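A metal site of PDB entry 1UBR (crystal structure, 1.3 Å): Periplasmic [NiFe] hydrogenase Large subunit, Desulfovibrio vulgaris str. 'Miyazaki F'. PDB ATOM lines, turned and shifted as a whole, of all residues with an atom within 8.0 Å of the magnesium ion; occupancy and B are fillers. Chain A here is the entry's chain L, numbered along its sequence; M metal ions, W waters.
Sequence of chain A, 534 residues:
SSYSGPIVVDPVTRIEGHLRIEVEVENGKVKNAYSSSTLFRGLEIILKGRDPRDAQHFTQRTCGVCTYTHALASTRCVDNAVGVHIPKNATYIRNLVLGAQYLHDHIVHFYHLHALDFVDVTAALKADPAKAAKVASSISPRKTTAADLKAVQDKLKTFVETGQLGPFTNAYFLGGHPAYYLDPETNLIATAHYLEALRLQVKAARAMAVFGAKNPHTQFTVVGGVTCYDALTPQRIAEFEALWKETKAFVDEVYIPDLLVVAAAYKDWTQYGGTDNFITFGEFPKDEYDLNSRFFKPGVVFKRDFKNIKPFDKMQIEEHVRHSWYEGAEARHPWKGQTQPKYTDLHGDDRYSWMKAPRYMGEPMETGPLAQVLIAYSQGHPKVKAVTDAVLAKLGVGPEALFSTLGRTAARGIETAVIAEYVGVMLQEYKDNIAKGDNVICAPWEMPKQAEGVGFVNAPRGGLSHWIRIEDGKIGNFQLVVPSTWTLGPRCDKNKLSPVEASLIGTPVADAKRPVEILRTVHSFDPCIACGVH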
ATOM      1  N   PHE A  40     -18.347 -16.585  17.485  1.00  0.00           N
ATOM      2  CA  PHE A  40     -18.184 -15.280  18.077  1.00  0.00           C
ATOM      3  C   PHE A  40     -18.670 -14.211  17.091  1.00  0.00           C
ATOM      4  O   PHE A  40     -18.375 -14.301  15.879  1.00  0.00           O
ATOM      5  CB  PHE A  40     -16.699 -15.067  18.404  1.00  0.00           C
ATOM      6  CG  PHE A  40     -16.389 -13.684  18.955  1.00  0.00           C
ATOM      7  CD1 PHE A  40     -16.642 -13.343  20.261  1.00  0.00           C
ATOM      8  CD2 PHE A  40     -15.792 -12.710  18.149  1.00  0.00           C
ATOM      9  CE1 PHE A  40     -16.333 -12.103  20.802  1.00  0.00           C
ATOM     10  CE2 PHE A  40     -15.474 -11.465  18.688  1.00  0.00           C
ATOM     11  CZ  PHE A  40     -15.704 -11.144  20.007  1.00  0.00           C
ATOM     12  N   GLU A  44     -20.077  -6.488  21.767  1.00  0.00           N
ATOM     13  CA  GLU A  44     -19.507  -5.515  22.698  1.00  0.00           C
ATOM     14  C   GLU A  44     -18.438  -4.654  22.064  1.00  0.00           C
ATOM     15  O   GLU A  44     -18.314  -3.476  22.360  1.00  0.00           O
ATOM     16  CB  GLU A  44     -18.933  -6.228  23.934  1.00  0.00           C
ATOM     17  CG  GLU A  44     -20.046  -6.909  24.790  1.00  0.00           C
ATOM     18  CD  GLU A  44     -19.514  -8.129  25.531  1.00  0.00           C
ATOM     19  OE1 GLU A  44     -18.446  -8.655  25.154  1.00  0.00           O
ATOM     20  OE2 GLU A  44     -20.224  -8.576  26.447  1.00  0.00           O
ATOM     21  N   GLU A 319     -16.092 -12.206  35.146  1.00  0.00           N
ATOM     22  CA  GLU A 319     -16.068 -13.069  33.958  1.00  0.00           C
ATOM     23  C   GLU A 319     -14.624 -13.479  33.623  1.00  0.00           C
ATOM     24  O   GLU A 319     -13.777 -12.636  33.341  1.00  0.00           O
ATOM     25  CB  GLU A 319     -16.721 -12.422  32.742  1.00  0.00           C
ATOM     26  CG  GLU A 319     -18.212 -12.108  32.992  1.00  0.00           C
ATOM     27  CD  GLU A 319     -18.778 -11.613  31.680  1.00  0.00           C
ATOM     28  OE1 GLU A 319     -19.488 -12.399  30.993  1.00  0.00           O
ATOM     29  OE2 GLU A 319     -18.501 -10.447  31.326  1.00  0.00           O
ATOM     30  N   TYR A 326      -9.910 -15.606  24.593  1.00  0.00           N
ATOM     31  CA  TYR A 326      -9.662 -14.197  24.772  1.00  0.00           C
ATOM     32  C   TYR A 326      -8.246 -14.006  25.301  1.00  0.00           C
ATOM     33  O   TYR A 326      -7.618 -14.949  25.771  1.00  0.00           O
ATOM     34  CB  TYR A 326     -10.680 -13.504  25.718  1.00  0.00           C
ATOM     35  CG  TYR A 326     -12.074 -13.628  25.137  1.00  0.00           C
ATOM     36  CD1 TYR A 326     -12.921 -14.657  25.622  1.00  0.00           C
ATOM     37  CD2 TYR A 326     -12.540 -12.770  24.153  1.00  0.00           C
ATOM     38  CE1 TYR A 326     -14.212 -14.804  25.111  1.00  0.00           C
ATOM     39  CE2 TYR A 326     -13.832 -12.917  23.642  1.00  0.00           C
ATOM     40  CZ  TYR A 326     -14.649 -13.918  24.113  1.00  0.00           C
ATOM     41  OH  TYR A 326     -15.927 -14.060  23.583  1.00  0.00           O
ATOM     42  N   PRO A 334     -17.920  -6.759  35.037  1.00  0.00           N
ATOM     43  CA  PRO A 334     -18.320  -6.198  33.757  1.00  0.00           C
ATOM     44  C   PRO A 334     -18.225  -4.684  33.656  1.00  0.00           C
ATOM     45  O   PRO A 334     -18.151  -4.225  32.500  1.00  0.00           O
ATOM     46  CB  PRO A 334     -19.778  -6.650  33.609  1.00  0.00           C
ATOM     47  CG  PRO A 334     -20.089  -7.530  34.725  1.00  0.00           C
ATOM     48  CD  PRO A 334     -18.943  -7.591  35.675  1.00  0.00           C
ATOM     49  N   GLY A 337     -15.036  -4.648  32.073  1.00  0.00           N
ATOM     50  CA  GLY A 337     -14.949  -5.775  31.173  1.00  0.00           C
ATOM     51  C   GLY A 337     -14.018  -5.547  30.009  1.00  0.00           C
ATOM     52  O   GLY A 337     -13.732  -4.405  29.622  1.00  0.00           O
ATOM     53  N   GLN A 338     -13.585  -6.688  29.460  1.00  0.00           N
ATOM     54  CA  GLN A 338     -12.720  -6.657  28.294  1.00  0.00           C
ATOM     55  C   GLN A 338     -13.155  -7.722  27.314  1.00  0.00           C
ATOM     56  O   GLN A 338     -13.454  -8.835  27.795  1.00  0.00           O
ATOM     57  CB  GLN A 338     -11.252  -6.955  28.614  1.00  0.00           C
ATOM     58  CG  GLN A 338     -10.661  -5.912  29.591  1.00  0.00           C
ATOM     59  CD  GLN A 338      -9.206  -6.204  29.883  1.00  0.00           C
ATOM     60  OE1 GLN A 338      -8.333  -5.369  29.634  1.00  0.00           O
ATOM     61  NE2 GLN A 338      -8.995  -7.394  30.428  1.00  0.00           N
ATOM     62  N   THR A 339     -13.180  -7.394  26.042  1.00  0.00           N
ATOM     63  CA  THR A 339     -13.543  -8.405  25.038  1.00  0.00           C
ATOM     64  C   THR A 339     -12.494  -8.360  23.927  1.00  0.00           C
ATOM     65  O   THR A 339     -12.610  -7.579  22.971  1.00  0.00           O
ATOM     66  CB  THR A 339     -14.968  -8.150  24.530  1.00  0.00           C
ATOM     67  OG1 THR A 339     -15.819  -8.137  25.690  1.00  0.00           O
ATOM     68  CG2 THR A 339     -15.422  -9.252  23.579  1.00  0.00           C
ATOM     69  N   TRP A 354     -15.779 -19.697  22.966  1.00  0.00           N
ATOM     70  CA  TRP A 354     -15.923 -18.244  22.827  1.00  0.00           C
ATOM     71  C   TRP A 354     -16.742 -17.659  23.982  1.00  0.00           C
ATOM     72  O   TRP A 354     -16.833 -16.415  24.038  1.00  0.00           O
ATOM     73  CB  TRP A 354     -16.599 -17.880  21.499  1.00  0.00           C
ATOM     74  CG  TRP A 354     -15.688 -18.080  20.317  1.00  0.00           C
ATOM     75  CD1 TRP A 354     -15.776 -19.024  19.334  1.00  0.00           C
ATOM     76  CD2 TRP A 354     -14.514 -17.305  19.978  1.00  0.00           C
ATOM     77  NE1 TRP A 354     -14.747 -18.895  18.394  1.00  0.00           N
ATOM     78  CE2 TRP A 354     -13.963 -17.854  18.783  1.00  0.00           C
ATOM     79  CE3 TRP A 354     -13.908 -16.214  20.601  1.00  0.00           C
ATOM     80  CZ2 TRP A 354     -12.805 -17.288  18.214  1.00  0.00           C
ATOM     81  CZ3 TRP A 354     -12.765 -15.644  20.057  1.00  0.00           C
ATOM     82  CH2 TRP A 354     -12.248 -16.216  18.870  1.00  0.00           C
ATOM     83  N   MET A 355     -17.345 -18.468  24.869  1.00  0.00           N
ATOM     84  CA  MET A 355     -17.978 -17.859  26.032  1.00  0.00           C
ATOM     85  C   MET A 355     -16.938 -17.538  27.102  1.00  0.00           C
ATOM     86  O   MET A 355     -15.994 -18.318  27.334  1.00  0.00           O
ATOM     87  CB  MET A 355     -18.998 -18.818  26.655  1.00  0.00           C
ATOM     88  CG  MET A 355     -20.292 -18.904  25.823  1.00  0.00           C
ATOM     89  SD  MET A 355     -21.558 -19.659  26.899  1.00  0.00           S
ATOM     90  CE  MET A 355     -22.702 -20.315  25.682  1.00  0.00           C
ATOM     91  N   LYS A 356     -17.130 -16.402  27.779  1.00  0.00           N
ATOM     92  CA  LYS A 356     -16.439 -16.138  29.055  1.00  0.00           C
ATOM     93  C   LYS A 356     -17.074 -17.027  30.112  1.00  0.00           C
ATOM     94  O   LYS A 356     -18.109 -17.643  29.839  1.00  0.00           O
ATOM     95  CB  LYS A 356     -16.574 -14.690  29.454  1.00  0.00           C
ATOM     96  CG  LYS A 356     -15.980 -13.730  28.428  1.00  0.00           C
ATOM     97  CD  LYS A 356     -16.229 -12.266  28.814  1.00  0.00           C
ATOM     98  CE  LYS A 356     -15.594 -11.318  27.796  1.00  0.00           C
ATOM     99  NZ  LYS A 356     -16.087  -9.910  28.069  1.00  0.00           N
ATOM    100  N   PRO A 358     -18.528 -16.691  33.702  1.00  0.00           N
ATOM    101  CA  PRO A 358     -18.894 -15.844  34.838  1.00  0.00           C
ATOM    102  C   PRO A 358     -18.867 -16.655  36.122  1.00  0.00           C
ATOM    103  O   PRO A 358     -19.278 -17.822  36.157  1.00  0.00           O
ATOM    104  CB  PRO A 358     -20.351 -15.448  34.505  1.00  0.00           C
ATOM    105  CG  PRO A 358     -20.487 -15.685  33.024  1.00  0.00           C
ATOM    106  CD  PRO A 358     -19.653 -16.958  32.812  1.00  0.00           C
ATOM    107  N   SER A 465     -27.698  -9.437  32.497  1.00  0.00           N
ATOM    108  CA  SER A 465     -27.349  -8.078  32.902  1.00  0.00           C
ATOM    109  C   SER A 465     -26.565  -7.420  31.767  1.00  0.00           C
ATOM    110  O   SER A 465     -25.718  -8.043  31.132  1.00  0.00           O
ATOM    111  CB  SER A 465     -26.581  -8.083  34.240  1.00  0.00           C
ATOM    112  OG  SER A 465     -25.479  -8.964  34.217  1.00  0.00           O
ATOM    113  N   TRP A 467     -24.292  -3.846  31.108  1.00  0.00           N
ATOM    114  CA  TRP A 467     -23.512  -2.910  31.913  1.00  0.00           C
ATOM    115  C   TRP A 467     -22.873  -1.833  31.027  1.00  0.00           C
ATOM    116  O   TRP A 467     -22.194  -2.200  30.056  1.00  0.00           O
ATOM    117  CB  TRP A 467     -22.393  -3.691  32.611  1.00  0.00           C
ATOM    118  CG  TRP A 467     -22.847  -4.882  33.404  1.00  0.00           C
ATOM    119  CD1 TRP A 467     -23.273  -6.100  32.976  1.00  0.00           C
ATOM    120  CD2 TRP A 467     -22.880  -4.915  34.858  1.00  0.00           C
ATOM    121  NE1 TRP A 467     -23.569  -6.878  34.094  1.00  0.00           N
ATOM    122  CE2 TRP A 467     -23.341  -6.185  35.245  1.00  0.00           C
ATOM    123  CE3 TRP A 467     -22.562  -3.974  35.845  1.00  0.00           C
ATOM    124  CZ2 TRP A 467     -23.499  -6.557  36.589  1.00  0.00           C
ATOM    125  CZ3 TRP A 467     -22.705  -4.317  37.170  1.00  0.00           C
ATOM    126  CH2 TRP A 467     -23.171  -5.602  37.525  1.00  0.00           C
ATOM    127  N   PHE A 478     -19.379  -1.425  27.023  1.00  0.00           N
ATOM    128  CA  PHE A 478     -20.725  -2.011  27.134  1.00  0.00           C
ATOM    129  C   PHE A 478     -20.498  -3.519  27.281  1.00  0.00           C
ATOM    130  O   PHE A 478     -19.870  -4.066  26.374  1.00  0.00           O
ATOM    131  CB  PHE A 478     -21.608  -1.705  25.925  1.00  0.00           C
ATOM    132  CG  PHE A 478     -23.102  -1.869  26.247  1.00  0.00           C
ATOM    133  CD1 PHE A 478     -23.645  -3.142  26.364  1.00  0.00           C
ATOM    134  CD2 PHE A 478     -23.927  -0.796  26.408  1.00  0.00           C
ATOM    135  CE1 PHE A 478     -24.994  -3.290  26.661  1.00  0.00           C
ATOM    136  CE2 PHE A 478     -25.281  -0.906  26.706  1.00  0.00           C
ATOM    137  CZ  PHE A 478     -25.853  -2.187  26.861  1.00  0.00           C
ATOM    138  N   GLN A 479     -20.962  -4.081  28.372  1.00  0.00           N
ATOM    139  CA  GLN A 479     -20.720  -5.519  28.580  1.00  0.00           C
ATOM    140  C   GLN A 479     -22.044  -6.235  28.823  1.00  0.00           C
ATOM    141  O   GLN A 479     -22.840  -5.779  29.630  1.00  0.00           O
ATOM    142  CB  GLN A 479     -19.744  -5.734  29.738  1.00  0.00           C
ATOM    143  CG  GLN A 479     -18.317  -5.238  29.493  1.00  0.00           C
ATOM    144  CD  GLN A 479     -17.585  -6.054  28.431  1.00  0.00           C
ATOM    145  OE1 GLN A 479     -17.755  -7.283  28.399  1.00  0.00           O
ATOM    146  NE2 GLN A 479     -16.757  -5.371  27.646  1.00  0.00           N
ATOM    147  N   LEU A 480     -22.250  -7.348  28.113  1.00  0.00           N
ATOM    148  CA  LEU A 480     -23.379  -8.252  28.330  1.00  0.00           C
ATOM    149  C   LEU A 480     -22.908  -9.465  29.100  1.00  0.00           C
ATOM    150  O   LEU A 480     -21.890 -10.010  28.755  1.00  0.00           O
ATOM    151  CB  LEU A 480     -23.996  -8.790  27.035  1.00  0.00           C
ATOM    152  CG  LEU A 480     -24.437  -7.785  25.941  1.00  0.00           C
ATOM    153  CD1 LEU A 480     -25.450  -8.502  25.058  1.00  0.00           C
ATOM    154  CD2 LEU A 480     -24.967  -6.566  26.533  1.00  0.00           C
ATOM    155  N   VAL A 481     -23.617  -9.845  30.164  1.00  0.00           N
ATOM    156  CA  VAL A 481     -23.307 -11.059  30.899  1.00  0.00           C
ATOM    157  C   VAL A 481     -24.638 -11.793  30.841  1.00  0.00           C
ATOM    158  O   VAL A 481     -25.639 -11.308  31.392  1.00  0.00           O
ATOM    159  CB  VAL A 481     -22.947 -10.830  32.356  1.00  0.00           C
ATOM    160  CG1 VAL A 481     -22.520 -12.163  33.024  1.00  0.00           C
ATOM    161  CG2 VAL A 481     -21.820  -9.821  32.421  1.00  0.00           C
ATOM    162  N   VAL A 482     -24.704 -12.911  30.134  1.00  0.00           N
ATOM    163  CA  VAL A 482     -26.013 -13.421  29.724  1.00  0.00           C
ATOM    164  C   VAL A 482     -26.291 -14.769  30.377  1.00  0.00           C
ATOM    165  O   VAL A 482     -25.310 -15.449  30.769  1.00  0.00           O
ATOM    166  CB  VAL A 482     -25.975 -13.499  28.183  1.00  0.00           C
ATOM    167  CG1 VAL A 482     -27.287 -13.927  27.574  1.00  0.00           C
ATOM    168  CG2 VAL A 482     -25.619 -12.142  27.569  1.00  0.00           C
ATOM    169  N   THR A 485     -24.267 -17.657  29.356  1.00  0.00           N
ATOM    170  CA  THR A 485     -22.851 -17.510  29.670  1.00  0.00           C
ATOM    171  C   THR A 485     -22.579 -18.135  31.028  1.00  0.00           C
ATOM    172  O   THR A 485     -21.606 -18.889  31.179  1.00  0.00           O
ATOM    173  CB  THR A 485     -22.429 -16.020  29.726  1.00  0.00           C
ATOM    174  OG1 THR A 485     -23.079 -15.267  28.709  1.00  0.00           O
ATOM    175  CG2 THR A 485     -20.929 -15.899  29.532  1.00  0.00           C
ATOM    176  N   CYS A 531     -26.691 -15.845  22.576  1.00  0.00           N
ATOM    177  CA  CYS A 531     -26.790 -15.186  23.855  1.00  0.00           C
ATOM    178  C   CYS A 531     -25.487 -15.306  24.631  1.00  0.00           C
ATOM    179  O   CYS A 531     -24.923 -14.343  25.146  1.00  0.00           O
ATOM    180  CB  CYS A 531     -27.906 -15.805  24.711  1.00  0.00           C
ATOM    181  SG  CYS A 531     -29.470 -14.928  24.483  1.00  0.00           S
ATOM    182  N   GLY A 532     -24.983 -16.534  24.797  1.00  0.00           N
ATOM    183  CA  GLY A 532     -23.873 -16.702  25.714  1.00  0.00           C
ATOM    184  C   GLY A 532     -22.616 -16.010  25.284  1.00  0.00           C
ATOM    185  O   GLY A 532     -21.846 -15.551  26.141  1.00  0.00           O
ATOM    186  N   VAL A 533     -22.375 -15.972  23.972  1.00  0.00           N
ATOM    187  CA  VAL A 533     -21.140 -15.375  23.428  1.00  0.00           C
ATOM    188  C   VAL A 533     -21.278 -13.955  22.944  1.00  0.00           C
ATOM    189  O   VAL A 533     -20.385 -13.124  23.200  1.00  0.00           O
ATOM    190  CB  VAL A 533     -20.619 -16.154  22.200  1.00  0.00           C
ATOM    191  CG1 VAL A 533     -19.364 -15.488  21.635  1.00  0.00           C
ATOM    192  CG2 VAL A 533     -20.335 -17.607  22.574  1.00  0.00           C
ATOM    193  N   HIS A 534     -22.368 -13.596  22.282  1.00  0.00           N
ATOM    194  CA  HIS A 534     -22.586 -12.249  21.708  1.00  0.00           C
ATOM    195  C   HIS A 534     -21.333 -11.714  20.981  1.00  0.00           C
ATOM    196  O   HIS A 534     -20.747 -12.579  20.192  1.00  0.00           O
ATOM    197  CB  HIS A 534     -23.151 -11.206  22.703  1.00  0.00           C
ATOM    198  CG  HIS A 534     -22.606 -11.261  24.093  1.00  0.00           C
ATOM    199  ND1 HIS A 534     -22.984 -12.289  24.970  1.00  0.00           N
ATOM    200  CD2 HIS A 534     -21.638 -10.554  24.706  1.00  0.00           C
ATOM    201  CE1 HIS A 534     -22.298 -12.127  26.078  1.00  0.00           C
ATOM    202  NE2 HIS A 534     -21.487 -11.093  25.953  1.00  0.00           N
ATOM    203  OXT HIS A 534     -20.953 -10.584  21.075  1.00  0.00           O
HETATM  204 MG    MG M   1     -20.176 -10.410  27.511  1.00  0.00          MG
HETATM  205  O   HOH W   1     -18.990  -9.662  29.055  1.00  0.00           O
HETATM  206  O   HOH W   2     -18.452 -11.019  26.504  1.00  0.00           O
HETATM  207  O   HOH W   3     -19.982 -12.240  28.448  1.00  0.00           O
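The side-chain amino group (NZ) of Lys 356 is in salt-bridge range of the side-chain carboxylate (OE1) of Glu 44, 3.95 Å away.
OE1 of Glu 44 sits at hydrogen-bond distance from OG1 of Thr 339 (2.7 Å).
A ring nitrogen (ND1) of His 534 lies within hydrogen-bond range of the backbone carbonyl oxygen (O) of Cys 531 (2.8 Å).
The side-chain amide oxygen (OE1) of Gln 479 lies close to the side-chain carboxylate (OE2) of Glu 44 (3.4 Å).
Three residues have an atom within 4 Å of the magnesium ion: Glu 44, Leu 480 and His 534.
The nearest printed residue that does not touch the magnesium ion is Gln 479 (4.1 Å).
Water W3 binds the magnesium ion.
The magnesium ion is bound by water W1 (2.1 Å).
The magnesium ion is bound by water W2, 2.1 Å away.
OE2 of Glu 44 is bound to the magnesium ion, 2.1 Å away.
NE2 of His 534 is bound to the magnesium ion, 2.1 Å away.
The magnesium ion is bound by O of Leu 480.
The magnesium ion has six donor atoms within binding distance.
Water W2 bridges OE1 of Glu 44 (2.7 Å) and NZ of Lys 356 (3.0 Å).
Water W1 lies within hydrogen-bond range of the side-chain carboxylate (OE2) of Glu 319 (2.5 Å), the side-chain amide oxygen (OE1) of Gln 479 (2.8 Å) and the side-chain amino group (NZ) of Lys 356 (3.1 Å).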
